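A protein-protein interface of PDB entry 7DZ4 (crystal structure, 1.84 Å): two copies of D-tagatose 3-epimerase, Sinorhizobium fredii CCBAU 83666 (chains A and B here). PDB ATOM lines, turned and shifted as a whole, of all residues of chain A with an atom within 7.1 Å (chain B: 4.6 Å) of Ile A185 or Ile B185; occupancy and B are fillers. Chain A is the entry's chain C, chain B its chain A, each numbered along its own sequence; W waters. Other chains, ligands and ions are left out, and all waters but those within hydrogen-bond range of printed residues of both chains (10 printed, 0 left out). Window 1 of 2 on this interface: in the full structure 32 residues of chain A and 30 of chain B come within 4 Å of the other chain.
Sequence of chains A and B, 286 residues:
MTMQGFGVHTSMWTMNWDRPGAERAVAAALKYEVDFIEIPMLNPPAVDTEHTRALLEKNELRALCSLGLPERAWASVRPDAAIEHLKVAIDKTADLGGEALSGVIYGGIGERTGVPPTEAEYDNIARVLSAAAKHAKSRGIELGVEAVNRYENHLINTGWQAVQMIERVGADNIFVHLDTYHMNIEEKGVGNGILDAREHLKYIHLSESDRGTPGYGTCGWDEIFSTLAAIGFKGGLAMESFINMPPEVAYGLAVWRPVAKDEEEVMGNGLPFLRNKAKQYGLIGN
Arg A150 touches Tyr B181, and with the chains exchanged Tyr A181 touches Arg B150. Asn B184 touches its own counterpart, Asn A184. Ile A185 touches Asp B210, and with the chains exchanged Asp A210 touches Ile B185. Positions printed for both chains: 149, 150, 181, 182, 183, 184, 185, 186, 187, 209 and 210. Of the 19 pairs that touch across the chains among the printed residues, 12 have their exchanged pair printed and touching as well.
Water W10 lies within hydrogen-bond range of the side-chain carboxylate of Glu B186 (2.7 Å) and the guanidinium group of Arg A257 (2.9 Å). Water W6 bridges the backbone carbonyl oxygen of Asp B210 (2.8 Å) and the guanidinium group of Arg A150 (2.9 Å). Water W8 lies within hydrogen-bond range of O of Arg A257 (2.8 Å) and NH1 of Arg B150 (3.4 Å).
A ring nitrogen (ND1) of His B182 lies within hydrogen-bond range of the backbone NH (N) of Asn B149, 3.1 Å away. The side-chain amide oxygen (OD1) of Asn A149 sits at hydrogen-bond distance from the backbone NH (N) of Tyr A151 (2.9 Å). The side-chain carboxylate (OE2) of Glu A186 is in salt-bridge range of the guanidinium group (NE) of Arg A150 (2.7 Å). The side-chain carboxylate (OD1) of Asp A179 lies within hydrogen-bond range of the backbone NH (N) of Tyr A181, 2.9 Å away.
The side-chain amide nitrogen of Asn B149 lies within hydrogen-bond range of the side-chain hydroxyl of Tyr A151, at 3.1 Å. OH of Tyr A151 lies within hydrogen-bond range of OH of Tyr B181 (2.8 Å). O of Asn B184 lies within hydrogen-bond range of ND2 of Asn A184, 3.0 Å away. O of Asn B184 is in hydrogen-bond range of OG1 of Thr A218. The guanidinium group (NH2) of Arg A257 lies within salt-bridge range of the side-chain carboxylate (OE1) of Glu B186, 2.9 Å away. OD2 of Asp B210 lies within salt-bridge range of NZ of Lys A188, at 2.9 Å. O of Ser B209 sits close to O of Ile A185 (3.1 Å). The backbone carbonyl oxygen of Ser A209 lies close to the backbone carbonyl oxygen of Ile B185 (3.2 Å).
Among the printed residues, merely in contact across the chains: Arg A150 with Tyr B181 (3.8 Å), Arg A150 with Asp B210 (3.8 Å), Tyr A181 with Arg B150 (3.7 Å), Asn A184 with Ser B209 (3.6 Å), Ile A185 with Ile B185 (3.7 Å), Ile A185 with Asp B210 (3.7 Å), Ser A209 with Asn B184 (3.6 Å), Asp A210 with Arg B150 (3.7 Å), Asp A210 with Ile B185 (3.4 Å), Thr A218 with Glu B187 (3.8 Å) and Arg A257 with Arg B150 (3.5 Å).
Printed residues of chain B within 4 Å of Arg A150: Tyr B181 and Asp B210. Thr A180 touches none of the printed residues of chain B. Ile A185 touches just these residues of chain B: Ile B185 (3.7 Å), Ser B209 (3.1 Å) and Asp B210 (3.7 Å). Printed residues of chain B within 4 Å of Lys A188: Asp B210 (2.9 Å). Arg A211 touches none of the printed residues of chain B. Printed residues of chain A within 4 Å of Asn B149: Tyr A151 (3.1 Å). Of chain A, only Ile A185 (3.7 Å), Ser A209 (3.2 Å) and Asp A210 (3.4 Å) come within 4 Å of Ile B185. Of the printed residues of chain A, Glu B187 touches Thr A218 (3.8 Å). Of the printed residues of chain A, Ser B209 touches Asn A184 and Ile A185. The nearest residue of chain B that does not touch Ile A185 is Tyr B181 (4.4 Å). The nearest residue of chain A that does not touch Ile B185 is Tyr A181 (4.6 Å).
Of the 20 printed residues of chain A, 10 touch a printed residue of chain B. Hydrophobic or aromatic side chains of chain A within 4 Å of the printed part of chain B: Tyr A151, Tyr A181 and Ile A185. Along chain A the printed residues that touch a printed residue of chain B span positions 150 to 257. Of the 11 printed residues of chain B, 9 touch a printed residue of chain A. Printed residues of chain B that touch a printed residue of chain A: Asn B149, Arg B150, Tyr B181, Asn B184, Ile B185, Glu B186, Glu B187, Ser B209 and Asp B210. Hydrophobic or aromatic side chains of chain B within 4 Å of the printed part of chain A: Tyr B181 and Ile B185. Among the printed residues, 19 pairs touch across the chains. Among the printed residues, Asp or Glu carboxylates within 4 Å of a Lys or Arg side-chain nitrogen of the other chain: Lys A188 with Asp B210 (2.9 Å) and Arg A257 with Glu B186 (2.9 Å).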
ATOM      1  N   ASN A 149      25.280  14.813  16.933  1.00  0.00           N
ATOM      2  CA  ASN A 149      24.044  14.619  16.201  1.00  0.00           C
ATOM      3  C   ASN A 149      24.283  14.773  14.698  1.00  0.00           C
ATOM      4  O   ASN A 149      25.305  15.311  14.234  1.00  0.00           O
ATOM      5  CB  ASN A 149      22.945  15.570  16.698  1.00  0.00           C
ATOM      6  CG  ASN A 149      23.222  16.984  16.377  1.00  0.00           C
ATOM      7  OD1 ASN A 149      23.165  17.383  15.206  1.00  0.00           O
ATOM      8  ND2 ASN A 149      23.449  17.786  17.404  1.00  0.00           N
ATOM      9  N   ARG A 150      23.283  14.304  13.950  1.00  0.00           N
ATOM     10  CA  ARG A 150      23.336  14.229  12.494  1.00  0.00           C
ATOM     11  C   ARG A 150      23.690  15.537  11.828  1.00  0.00           C
ATOM     12  O   ARG A 150      24.245  15.531  10.714  1.00  0.00           O
ATOM     13  CB  ARG A 150      21.965  13.766  11.978  1.00  0.00           C
ATOM     14  CG  ARG A 150      20.809  14.714  12.352  1.00  0.00           C
ATOM     15  CD  ARG A 150      19.423  14.007  12.335  1.00  0.00           C
ATOM     16  NE  ARG A 150      19.405  12.833  13.187  1.00  0.00           N
ATOM     17  CZ  ARG A 150      18.464  11.902  13.155  1.00  0.00           C
ATOM     18  NH1 ARG A 150      17.440  12.003  12.320  1.00  0.00           N
ATOM     19  NH2 ARG A 150      18.544  10.872  13.961  1.00  0.00           N
ATOM     20  N   TYR A 151      23.338  16.659  12.447  1.00  0.00           N
ATOM     21  CA  TYR A 151      23.584  17.942  11.834  1.00  0.00           C
ATOM     22  C   TYR A 151      24.998  18.443  12.033  1.00  0.00           C
ATOM     23  O   TYR A 151      25.423  19.351  11.305  1.00  0.00           O
ATOM     24  CB  TYR A 151      22.644  19.008  12.380  1.00  0.00           C
ATOM     25  CG  TYR A 151      21.173  18.720  12.202  1.00  0.00           C
ATOM     26  CD1 TYR A 151      20.560  18.836  10.964  1.00  0.00           C
ATOM     27  CD2 TYR A 151      20.379  18.371  13.305  1.00  0.00           C
ATOM     28  CE1 TYR A 151      19.210  18.617  10.814  1.00  0.00           C
ATOM     29  CE2 TYR A 151      19.041  18.162  13.160  1.00  0.00           C
ATOM     30  CZ  TYR A 151      18.447  18.264  11.912  1.00  0.00           C
ATOM     31  OH  TYR A 151      17.085  18.051  11.782  1.00  0.00           O
ATOM     32  N   ASN A 157      27.085   9.119  15.169  1.00  0.00           N
ATOM     33  CA  ASN A 157      25.987   9.858  15.733  1.00  0.00           C
ATOM     34  C   ASN A 157      25.396   9.197  16.966  1.00  0.00           C
ATOM     35  O   ASN A 157      24.684   9.866  17.698  1.00  0.00           O
ATOM     36  CB  ASN A 157      24.839  10.015  14.732  1.00  0.00           C
ATOM     37  CG  ASN A 157      25.201  10.764  13.491  1.00  0.00           C
ATOM     38  OD1 ASN A 157      24.658  10.463  12.441  1.00  0.00           O
ATOM     39  ND2 ASN A 157      26.019  11.795  13.606  1.00  0.00           N
ATOM     40  N   ASP A 179      27.047  12.418  24.768  1.00  0.00           N
ATOM     41  CA  ASP A 179      26.596  13.764  25.089  1.00  0.00           C
ATOM     42  C   ASP A 179      25.079  13.788  25.095  1.00  0.00           C
ATOM     43  O   ASP A 179      24.447  13.391  24.115  1.00  0.00           O
ATOM     44  CB  ASP A 179      27.205  14.737  24.063  1.00  0.00           C
ATOM     45  CG  ASP A 179      26.861  16.155  24.316  1.00  0.00           C
ATOM     46  OD1 ASP A 179      25.709  16.402  24.617  1.00  0.00           O
ATOM     47  OD2 ASP A 179      27.755  17.061  24.161  1.00  0.00           O
ATOM     48  N   THR A 180      24.485  14.173  26.238  1.00  0.00           N
ATOM     49  CA  THR A 180      23.037  14.029  26.379  1.00  0.00           C
ATOM     50  C   THR A 180      22.280  14.954  25.433  1.00  0.00           C
ATOM     51  O   THR A 180      21.214  14.577  24.932  1.00  0.00           O
ATOM     52  CB  THR A 180      22.623  14.246  27.840  1.00  0.00           C
ATOM     53  OG1 THR A 180      23.033  15.555  28.283  1.00  0.00           O
ATOM     54  CG2 THR A 180      23.245  13.156  28.743  1.00  0.00           C
ATOM     55  N   TYR A 181      22.874  16.114  25.061  1.00  0.00           N
ATOM     56  CA  TYR A 181      22.279  16.952  24.023  1.00  0.00           C
ATOM     57  C   TYR A 181      22.206  16.233  22.679  1.00  0.00           C
ATOM     58  O   TYR A 181      21.184  16.301  21.967  1.00  0.00           O
ATOM     59  CB  TYR A 181      23.105  18.238  23.907  1.00  0.00           C
ATOM     60  CG  TYR A 181      22.870  19.052  22.689  1.00  0.00           C
ATOM     61  CD1 TYR A 181      21.875  19.997  22.664  1.00  0.00           C
ATOM     62  CD2 TYR A 181      23.683  18.913  21.561  1.00  0.00           C
ATOM     63  CE1 TYR A 181      21.676  20.804  21.581  1.00  0.00           C
ATOM     64  CE2 TYR A 181      23.475  19.691  20.447  1.00  0.00           C
ATOM     65  CZ  TYR A 181      22.476  20.649  20.470  1.00  0.00           C
ATOM     66  OH  TYR A 181      22.286  21.449  19.395  1.00  0.00           O
ATOM     67  N   HIS A 182      23.249  15.494  22.336  1.00  0.00           N
ATOM     68  CA  HIS A 182      23.235  14.785  21.066  1.00  0.00           C
ATOM     69  C   HIS A 182      22.379  13.544  21.163  1.00  0.00           C
ATOM     70  O   HIS A 182      21.652  13.219  20.228  1.00  0.00           O
ATOM     71  CB  HIS A 182      24.628  14.379  20.667  1.00  0.00           C
ATOM     72  CG  HIS A 182      25.499  15.539  20.373  1.00  0.00           C
ATOM     73  ND1 HIS A 182      25.157  16.499  19.443  1.00  0.00           N
ATOM     74  CD2 HIS A 182      26.682  15.926  20.911  1.00  0.00           C
ATOM     75  CE1 HIS A 182      26.104  17.425  19.413  1.00  0.00           C
ATOM     76  NE2 HIS A 182      27.055  17.088  20.272  1.00  0.00           N
ATOM     77  N   MET A 183      22.427  12.874  22.320  1.00  0.00           N
ATOM     78  CA  MET A 183      21.620  11.680  22.493  1.00  0.00           C
ATOM     79  C   MET A 183      20.147  12.011  22.463  1.00  0.00           C
ATOM     80  O   MET A 183      19.352  11.224  21.926  1.00  0.00           O
ATOM     81  CB  MET A 183      22.017  10.999  23.786  1.00  0.00           C
ATOM     82  CG  MET A 183      23.318  10.257  23.623  1.00  0.00           C
ATOM     83  SD  MET A 183      23.566   9.149  25.057  1.00  0.00           S
ATOM     84  CE  MET A 183      23.784  10.351  26.312  1.00  0.00           C
ATOM     85  N   ASN A 184      19.781  13.180  22.987  1.00  0.00           N
ATOM     86  CA  ASN A 184      18.405  13.646  22.944  1.00  0.00           C
ATOM     87  C   ASN A 184      17.839  13.656  21.533  1.00  0.00           C
ATOM     88  O   ASN A 184      16.612  13.531  21.359  1.00  0.00           O
ATOM     89  CB  ASN A 184      18.313  15.063  23.511  1.00  0.00           C
ATOM     90  CG  ASN A 184      16.906  15.536  23.689  1.00  0.00           C
ATOM     91  OD1 ASN A 184      16.098  14.862  24.344  1.00  0.00           O
ATOM     92  ND2 ASN A 184      16.602  16.723  23.157  1.00  0.00           N
ATOM     93  N   ILE A 185      18.698  13.882  20.531  1.00  0.00           N
ATOM     94  CA  ILE A 185      18.318  13.809  19.119  1.00  0.00           C
ATOM     95  C   ILE A 185      18.497  12.406  18.555  1.00  0.00           C
ATOM     96  O   ILE A 185      17.633  11.921  17.844  1.00  0.00           O
ATOM     97  CB  ILE A 185      19.149  14.825  18.292  1.00  0.00           C
ATOM     98  CG1 ILE A 185      18.972  16.228  18.826  1.00  0.00           C
ATOM     99  CG2 ILE A 185      18.756  14.748  16.858  1.00  0.00           C
ATOM    100  CD1 ILE A 185      19.984  17.203  18.199  1.00  0.00           C
ATOM    101  N   GLU A 186      19.609  11.719  18.840  1.00  0.00           N
ATOM    102  CA  GLU A 186      19.977  10.549  18.054  1.00  0.00           C
ATOM    103  C   GLU A 186      19.553   9.201  18.612  1.00  0.00           C
ATOM    104  O   GLU A 186      19.438   8.246  17.837  1.00  0.00           O
ATOM    105  CB  GLU A 186      21.489  10.468  17.872  1.00  0.00           C
ATOM    106  CG  GLU A 186      22.022  11.652  17.099  1.00  0.00           C
ATOM    107  CD  GLU A 186      21.498  11.718  15.638  1.00  0.00           C
ATOM    108  OE1 GLU A 186      21.259  10.653  15.031  1.00  0.00           O
ATOM    109  OE2 GLU A 186      21.288  12.854  15.143  1.00  0.00           O
ATOM    110  N   GLU A 187      19.419   9.061  19.929  1.00  0.00           N
ATOM    111  CA  GLU A 187      19.218   7.752  20.527  1.00  0.00           C
ATOM    112  C   GLU A 187      17.730   7.468  20.603  1.00  0.00           C
ATOM    113  O   GLU A 187      16.913   8.345  20.928  1.00  0.00           O
ATOM    114  CB  GLU A 187      19.836   7.680  21.920  1.00  0.00           C
ATOM    115  CG  GLU A 187      21.320   7.956  21.970  1.00  0.00           C
ATOM    116  CD  GLU A 187      22.175   6.904  21.264  1.00  0.00           C
ATOM    117  OE1 GLU A 187      21.654   5.814  20.861  1.00  0.00           O
ATOM    118  OE2 GLU A 187      23.376   7.187  21.091  1.00  0.00           O
ATOM    119  N   LYS A 188      17.377   6.216  20.348  1.00  0.00           N
ATOM    120  CA  LYS A 188      15.975   5.817  20.321  1.00  0.00           C
ATOM    121  C   LYS A 188      15.590   5.455  21.746  1.00  0.00           C
ATOM    122  O   LYS A 188      15.486   4.286  22.127  1.00  0.00           O
ATOM    123  CB  LYS A 188      15.770   4.666  19.354  1.00  0.00           C
ATOM    124  CG  LYS A 188      14.335   4.608  18.887  1.00  0.00           C
ATOM    125  CD  LYS A 188      14.064   3.328  18.126  1.00  0.00           C
ATOM    126  CE  LYS A 188      14.340   3.484  16.649  1.00  0.00           C
ATOM    127  NZ  LYS A 188      13.471   4.527  16.011  1.00  0.00           N
ATOM    128  N   GLU A 208      22.157  20.115  28.507  1.00  0.00           N
ATOM    129  CA  GLU A 208      20.717  20.203  28.279  1.00  0.00           C
ATOM    130  C   GLU A 208      20.395  20.229  26.781  1.00  0.00           C
ATOM    131  O   GLU A 208      21.206  20.633  25.922  1.00  0.00           O
ATOM    132  CB  GLU A 208      20.138  21.444  28.949  1.00  0.00           C
ATOM    133  CG  GLU A 208      18.619  21.446  29.168  1.00  0.00           C
ATOM    134  CD  GLU A 208      18.064  20.111  29.649  1.00  0.00           C
ATOM    135  OE1 GLU A 208      17.986  19.932  30.874  1.00  0.00           O
ATOM    136  OE2 GLU A 208      17.678  19.256  28.811  1.00  0.00           O
ATOM    137  N   SER A 209      19.143  19.884  26.496  1.00  0.00           N
ATOM    138  CA  SER A 209      18.647  19.730  25.142  1.00  0.00           C
ATOM    139  C   SER A 209      18.845  20.971  24.282  1.00  0.00           C
ATOM    140  O   SER A 209      18.967  20.848  23.057  1.00  0.00           O
ATOM    141  CB  SER A 209      17.148  19.389  25.177  1.00  0.00           C
ATOM    142  OG  SER A 209      16.446  20.327  25.986  1.00  0.00           O
ATOM    143  N   ASP A 210      18.838  22.165  24.874  1.00  0.00           N
ATOM    144  CA  ASP A 210      19.055  23.404  24.121  1.00  0.00           C
ATOM    145  C   ASP A 210      20.408  24.064  24.441  1.00  0.00           C
ATOM    146  O   ASP A 210      20.602  25.244  24.153  1.00  0.00           O
ATOM    147  CB  ASP A 210      17.913  24.377  24.398  1.00  0.00           C
ATOM    148  CG  ASP A 210      17.866  24.833  25.853  1.00  0.00           C
ATOM    149  OD1 ASP A 210      18.560  24.243  26.700  1.00  0.00           O
ATOM    150  OD2 ASP A 210      17.133  25.805  26.166  1.00  0.00           O
ATOM    151  N   ARG A 211      21.339  23.290  25.000  1.00  0.00           N
ATOM    152  CA  ARG A 211      22.644  23.703  25.502  1.00  0.00           C
ATOM    153  C   ARG A 211      22.565  24.643  26.693  1.00  0.00           C
ATOM    154  O   ARG A 211      23.574  25.267  27.073  1.00  0.00           O
ATOM    155  CB  ARG A 211      23.500  24.310  24.389  1.00  0.00           C
ATOM    156  CG  ARG A 211      23.850  23.325  23.316  1.00  0.00           C
ATOM    157  CD  ARG A 211      24.723  22.205  23.818  1.00  0.00           C
ATOM    158  NE  ARG A 211      25.472  21.621  22.717  1.00  0.00           N
ATOM    159  CZ  ARG A 211      26.247  20.539  22.822  1.00  0.00           C
ATOM    160  NH1 ARG A 211      26.354  19.906  23.979  1.00  0.00           N
ATOM    161  NH2 ARG A 211      26.920  20.093  21.763  1.00  0.00           N
ATOM    162  N   THR A 218      14.590  19.286  27.748  1.00  0.00           N
ATOM    163  CA  THR A 218      13.844  18.090  27.404  1.00  0.00           C
ATOM    164  C   THR A 218      14.643  16.818  27.586  1.00  0.00           C
ATOM    165  O   THR A 218      14.142  15.746  27.240  1.00  0.00           O
ATOM    166  CB  THR A 218      13.365  18.167  25.957  1.00  0.00           C
ATOM    167  OG1 THR A 218      14.497  17.961  25.088  1.00  0.00           O
ATOM    168  CG2 THR A 218      12.755  19.536  25.680  1.00  0.00           C
ATOM    169  N   ARG A 257      21.356  32.264  19.577  1.00  0.00           N
ATOM    170  CA  ARG A 257      20.705  33.035  20.623  1.00  0.00           C
ATOM    171  C   ARG A 257      21.198  32.493  21.944  1.00  0.00           C
ATOM    172  O   ARG A 257      21.682  31.348  22.000  1.00  0.00           O
ATOM    173  CB  ARG A 257      19.181  32.898  20.533  1.00  0.00           C
ATOM    174  CG  ARG A 257      18.759  31.459  20.500  1.00  0.00           C
ATOM    175  CD  ARG A 257      17.281  31.293  20.191  1.00  0.00           C
ATOM    176  NE  ARG A 257      16.883  29.886  20.248  1.00  0.00           N
ATOM    177  CZ  ARG A 257      16.420  29.266  21.330  1.00  0.00           C
ATOM    178  NH1 ARG A 257      16.287  29.906  22.487  1.00  0.00           N
ATOM    179  NH2 ARG A 257      16.086  27.987  21.230  1.00  0.00           N
ATOM    180  N   ASN B 149      14.512  23.553  13.723  1.00  0.00           N
ATOM    181  CA  ASN B 149      15.623  23.696  14.648  1.00  0.00           C
ATOM    182  C   ASN B 149      16.784  24.514  14.063  1.00  0.00           C
ATOM    183  O   ASN B 149      16.935  24.706  12.842  1.00  0.00           O
ATOM    184  CB  ASN B 149      16.165  22.335  15.120  1.00  0.00           C
ATOM    185  CG  ASN B 149      16.854  21.561  14.038  1.00  0.00           C
ATOM    186  OD1 ASN B 149      17.939  21.912  13.591  1.00  0.00           O
ATOM    187  ND2 ASN B 149      16.217  20.458  13.602  1.00  0.00           N
ATOM    188  N   ARG B 150      17.667  24.901  14.988  1.00  0.00           N
ATOM    189  CA  ARG B 150      18.820  25.755  14.720  1.00  0.00           C
ATOM    190  C   ARG B 150      19.676  25.320  13.548  1.00  0.00           C
ATOM    191  O   ARG B 150      20.347  26.160  12.913  1.00  0.00           O
ATOM    192  CB  ARG B 150      19.675  25.776  15.999  1.00  0.00           C
ATOM    193  CG  ARG B 150      20.198  24.384  16.437  1.00  0.00           C
ATOM    194  CD  ARG B 150      20.684  24.423  17.887  1.00  0.00           C
ATOM    195  NE  ARG B 150      19.611  24.860  18.775  1.00  0.00           N
ATOM    196  CZ  ARG B 150      19.798  25.329  20.003  1.00  0.00           C
ATOM    197  NH1 ARG B 150      21.009  25.421  20.524  1.00  0.00           N
ATOM    198  NH2 ARG B 150      18.776  25.752  20.689  1.00  0.00           N
ATOM    199  N   TYR B 181       9.557  17.406  17.058  1.00  0.00           N
ATOM    200  CA  TYR B 181      10.954  17.054  16.860  1.00  0.00           C
ATOM    201  C   TYR B 181      11.846  18.286  16.961  1.00  0.00           C
ATOM    202  O   TYR B 181      12.946  18.234  17.529  1.00  0.00           O
ATOM    203  CB  TYR B 181      11.104  16.370  15.481  1.00  0.00           C
ATOM    204  CG  TYR B 181      12.519  16.296  14.945  1.00  0.00           C
ATOM    205  CD1 TYR B 181      13.069  17.335  14.204  1.00  0.00           C
ATOM    206  CD2 TYR B 181      13.290  15.156  15.154  1.00  0.00           C
ATOM    207  CE1 TYR B 181      14.340  17.240  13.681  1.00  0.00           C
ATOM    208  CE2 TYR B 181      14.538  15.051  14.646  1.00  0.00           C
ATOM    209  CZ  TYR B 181      15.069  16.101  13.926  1.00  0.00           C
ATOM    210  OH  TYR B 181      16.306  15.958  13.426  1.00  0.00           O
ATOM    211  N   HIS B 182      11.391  19.417  16.434  1.00  0.00           N
ATOM    212  CA  HIS B 182      12.210  20.624  16.537  1.00  0.00           C
ATOM    213  C   HIS B 182      12.121  21.213  17.934  1.00  0.00           C
ATOM    214  O   HIS B 182      13.127  21.710  18.468  1.00  0.00           O
ATOM    215  CB  HIS B 182      11.771  21.651  15.514  1.00  0.00           C
ATOM    216  CG  HIS B 182      11.960  21.200  14.091  1.00  0.00           C
ATOM    217  ND1 HIS B 182      13.179  20.811  13.581  1.00  0.00           N
ATOM    218  CD2 HIS B 182      11.067  21.043  13.097  1.00  0.00           C
ATOM    219  CE1 HIS B 182      13.023  20.415  12.326  1.00  0.00           C
ATOM    220  NE2 HIS B 182      11.752  20.573  12.000  1.00  0.00           N
ATOM    221  N   MET B 183      10.926  21.151  18.539  1.00  0.00           N
ATOM    222  CA  MET B 183      10.748  21.664  19.903  1.00  0.00           C
ATOM    223  C   MET B 183      11.581  20.889  20.892  1.00  0.00           C
ATOM    224  O   MET B 183      12.076  21.453  21.876  1.00  0.00           O
ATOM    225  CB  MET B 183       9.283  21.576  20.307  1.00  0.00           C
ATOM    226  CG  MET B 183       8.421  22.623  19.681  1.00  0.00           C
ATOM    227  SD  MET B 183       6.797  22.760  20.403  1.00  0.00           S
ATOM    228  CE  MET B 183       6.255  21.288  19.701  1.00  0.00           C
ATOM    229  N   ASN B 184      11.724  19.591  20.646  1.00  0.00           N
ATOM    230  CA  ASN B 184      12.547  18.730  21.478  1.00  0.00           C
ATOM    231  C   ASN B 184      13.973  19.247  21.589  1.00  0.00           C
ATOM    232  O   ASN B 184      14.662  18.954  22.569  1.00  0.00           O
ATOM    233  CB  ASN B 184      12.500  17.295  20.919  1.00  0.00           C
ATOM    234  CG  ASN B 184      13.201  16.299  21.810  1.00  0.00           C
ATOM    235  OD1 ASN B 184      14.137  15.584  21.390  1.00  0.00           O
ATOM    236  ND2 ASN B 184      12.763  16.240  23.040  1.00  0.00           N
ATOM    237  N   ILE B 185      14.441  19.997  20.592  1.00  0.00           N
ATOM    238  CA  ILE B 185      15.749  20.616  20.622  1.00  0.00           C
ATOM    239  C   ILE B 185      15.662  22.057  21.110  1.00  0.00           C
ATOM    240  O   ILE B 185      16.475  22.493  21.919  1.00  0.00           O
ATOM    241  CB  ILE B 185      16.400  20.555  19.214  1.00  0.00           C
ATOM    242  CG1 ILE B 185      16.608  19.107  18.726  1.00  0.00           C
ATOM    243  CG2 ILE B 185      17.735  21.320  19.204  1.00  0.00           C
ATOM    244  CD1 ILE B 185      16.750  18.954  17.215  1.00  0.00           C
ATOM    245  N   GLU B 186      14.680  22.815  20.619  1.00  0.00           N
ATOM    246  CA  GLU B 186      14.708  24.264  20.764  1.00  0.00           C
ATOM    247  C   GLU B 186      14.022  24.822  22.008  1.00  0.00           C
ATOM    248  O   GLU B 186      14.405  25.910  22.476  1.00  0.00           O
ATOM    249  CB  GLU B 186      14.040  24.907  19.555  1.00  0.00           C
ATOM    250  CG  GLU B 186      14.755  24.621  18.252  1.00  0.00           C
ATOM    251  CD  GLU B 186      16.173  25.171  18.238  1.00  0.00           C
ATOM    252  OE1 GLU B 186      16.393  26.226  18.895  1.00  0.00           O
ATOM    253  OE2 GLU B 186      17.067  24.549  17.594  1.00  0.00           O
ATOM    254  N   GLU B 187      12.982  24.166  22.510  1.00  0.00           N
ATOM    255  CA  GLU B 187      12.173  24.772  23.571  1.00  0.00           C
ATOM    256  C   GLU B 187      12.738  24.426  24.940  1.00  0.00           C
ATOM    257  O   GLU B 187      13.132  23.282  25.193  1.00  0.00           O
ATOM    258  CB  GLU B 187      10.722  24.331  23.499  1.00  0.00           C
ATOM    259  CG  GLU B 187      10.016  24.645  22.136  1.00  0.00           C
ATOM    260  CD  GLU B 187       9.914  26.131  21.782  1.00  0.00           C
ATOM    261  OE1 GLU B 187      10.171  27.021  22.635  1.00  0.00           O
ATOM    262  OE2 GLU B 187       9.550  26.416  20.617  1.00  0.00           O
ATOM    263  N   SER B 209      11.604  12.236  18.436  1.00  0.00           N
ATOM    264  CA  SER B 209      12.881  12.939  18.530  1.00  0.00           C
ATOM    265  C   SER B 209      13.923  12.492  17.510  1.00  0.00           C
ATOM    266  O   SER B 209      14.877  13.245  17.262  1.00  0.00           O
ATOM    267  CB  SER B 209      13.445  12.733  19.923  1.00  0.00           C
ATOM    268  OG  SER B 209      13.466  11.362  20.213  1.00  0.00           O
ATOM    269  N   ASP B 210      13.800  11.273  16.970  1.00  0.00           N
ATOM    270  CA  ASP B 210      14.704  10.743  15.943  1.00  0.00           C
ATOM    271  C   ASP B 210      14.019  10.591  14.585  1.00  0.00           C
ATOM    272  O   ASP B 210      14.568   9.943  13.692  1.00  0.00           O
ATOM    273  CB  ASP B 210      15.286   9.382  16.388  1.00  0.00           C
ATOM    274  CG  ASP B 210      14.221   8.281  16.490  1.00  0.00           C
ATOM    275  OD1 ASP B 210      13.024   8.593  16.402  1.00  0.00           O
ATOM    276  OD2 ASP B 210      14.592   7.102  16.642  1.00  0.00           O
HETATM  277  O   HOH W   1      19.396  27.367  23.101  1.00  0.00           O
HETATM  278  O   HOH W   2      23.433  24.043  19.764  1.00  0.00           O
HETATM  279  O   HOH W   3      11.568   6.280  17.225  1.00  0.00           O
HETATM  280  O   HOH W   4      16.700  14.066  10.547  1.00  0.00           O
HETATM  281  O   HOH W   5      15.603  27.392  24.370  1.00  0.00           O
HETATM  282  O   HOH W   6      16.970   8.544  13.303  1.00  0.00           O
HETATM  283  O   HOH W   7      15.846  10.473  19.736  1.00  0.00           O
HETATM  284  O   HOH W   8      20.848  28.709  21.475  1.00  0.00           O
HETATM  285  O   HOH W   9      15.338  22.056  24.530  1.00  0.00           O
HETATM  286  O   HOH W  10      17.938  28.310  18.059  1.00  0.00           O
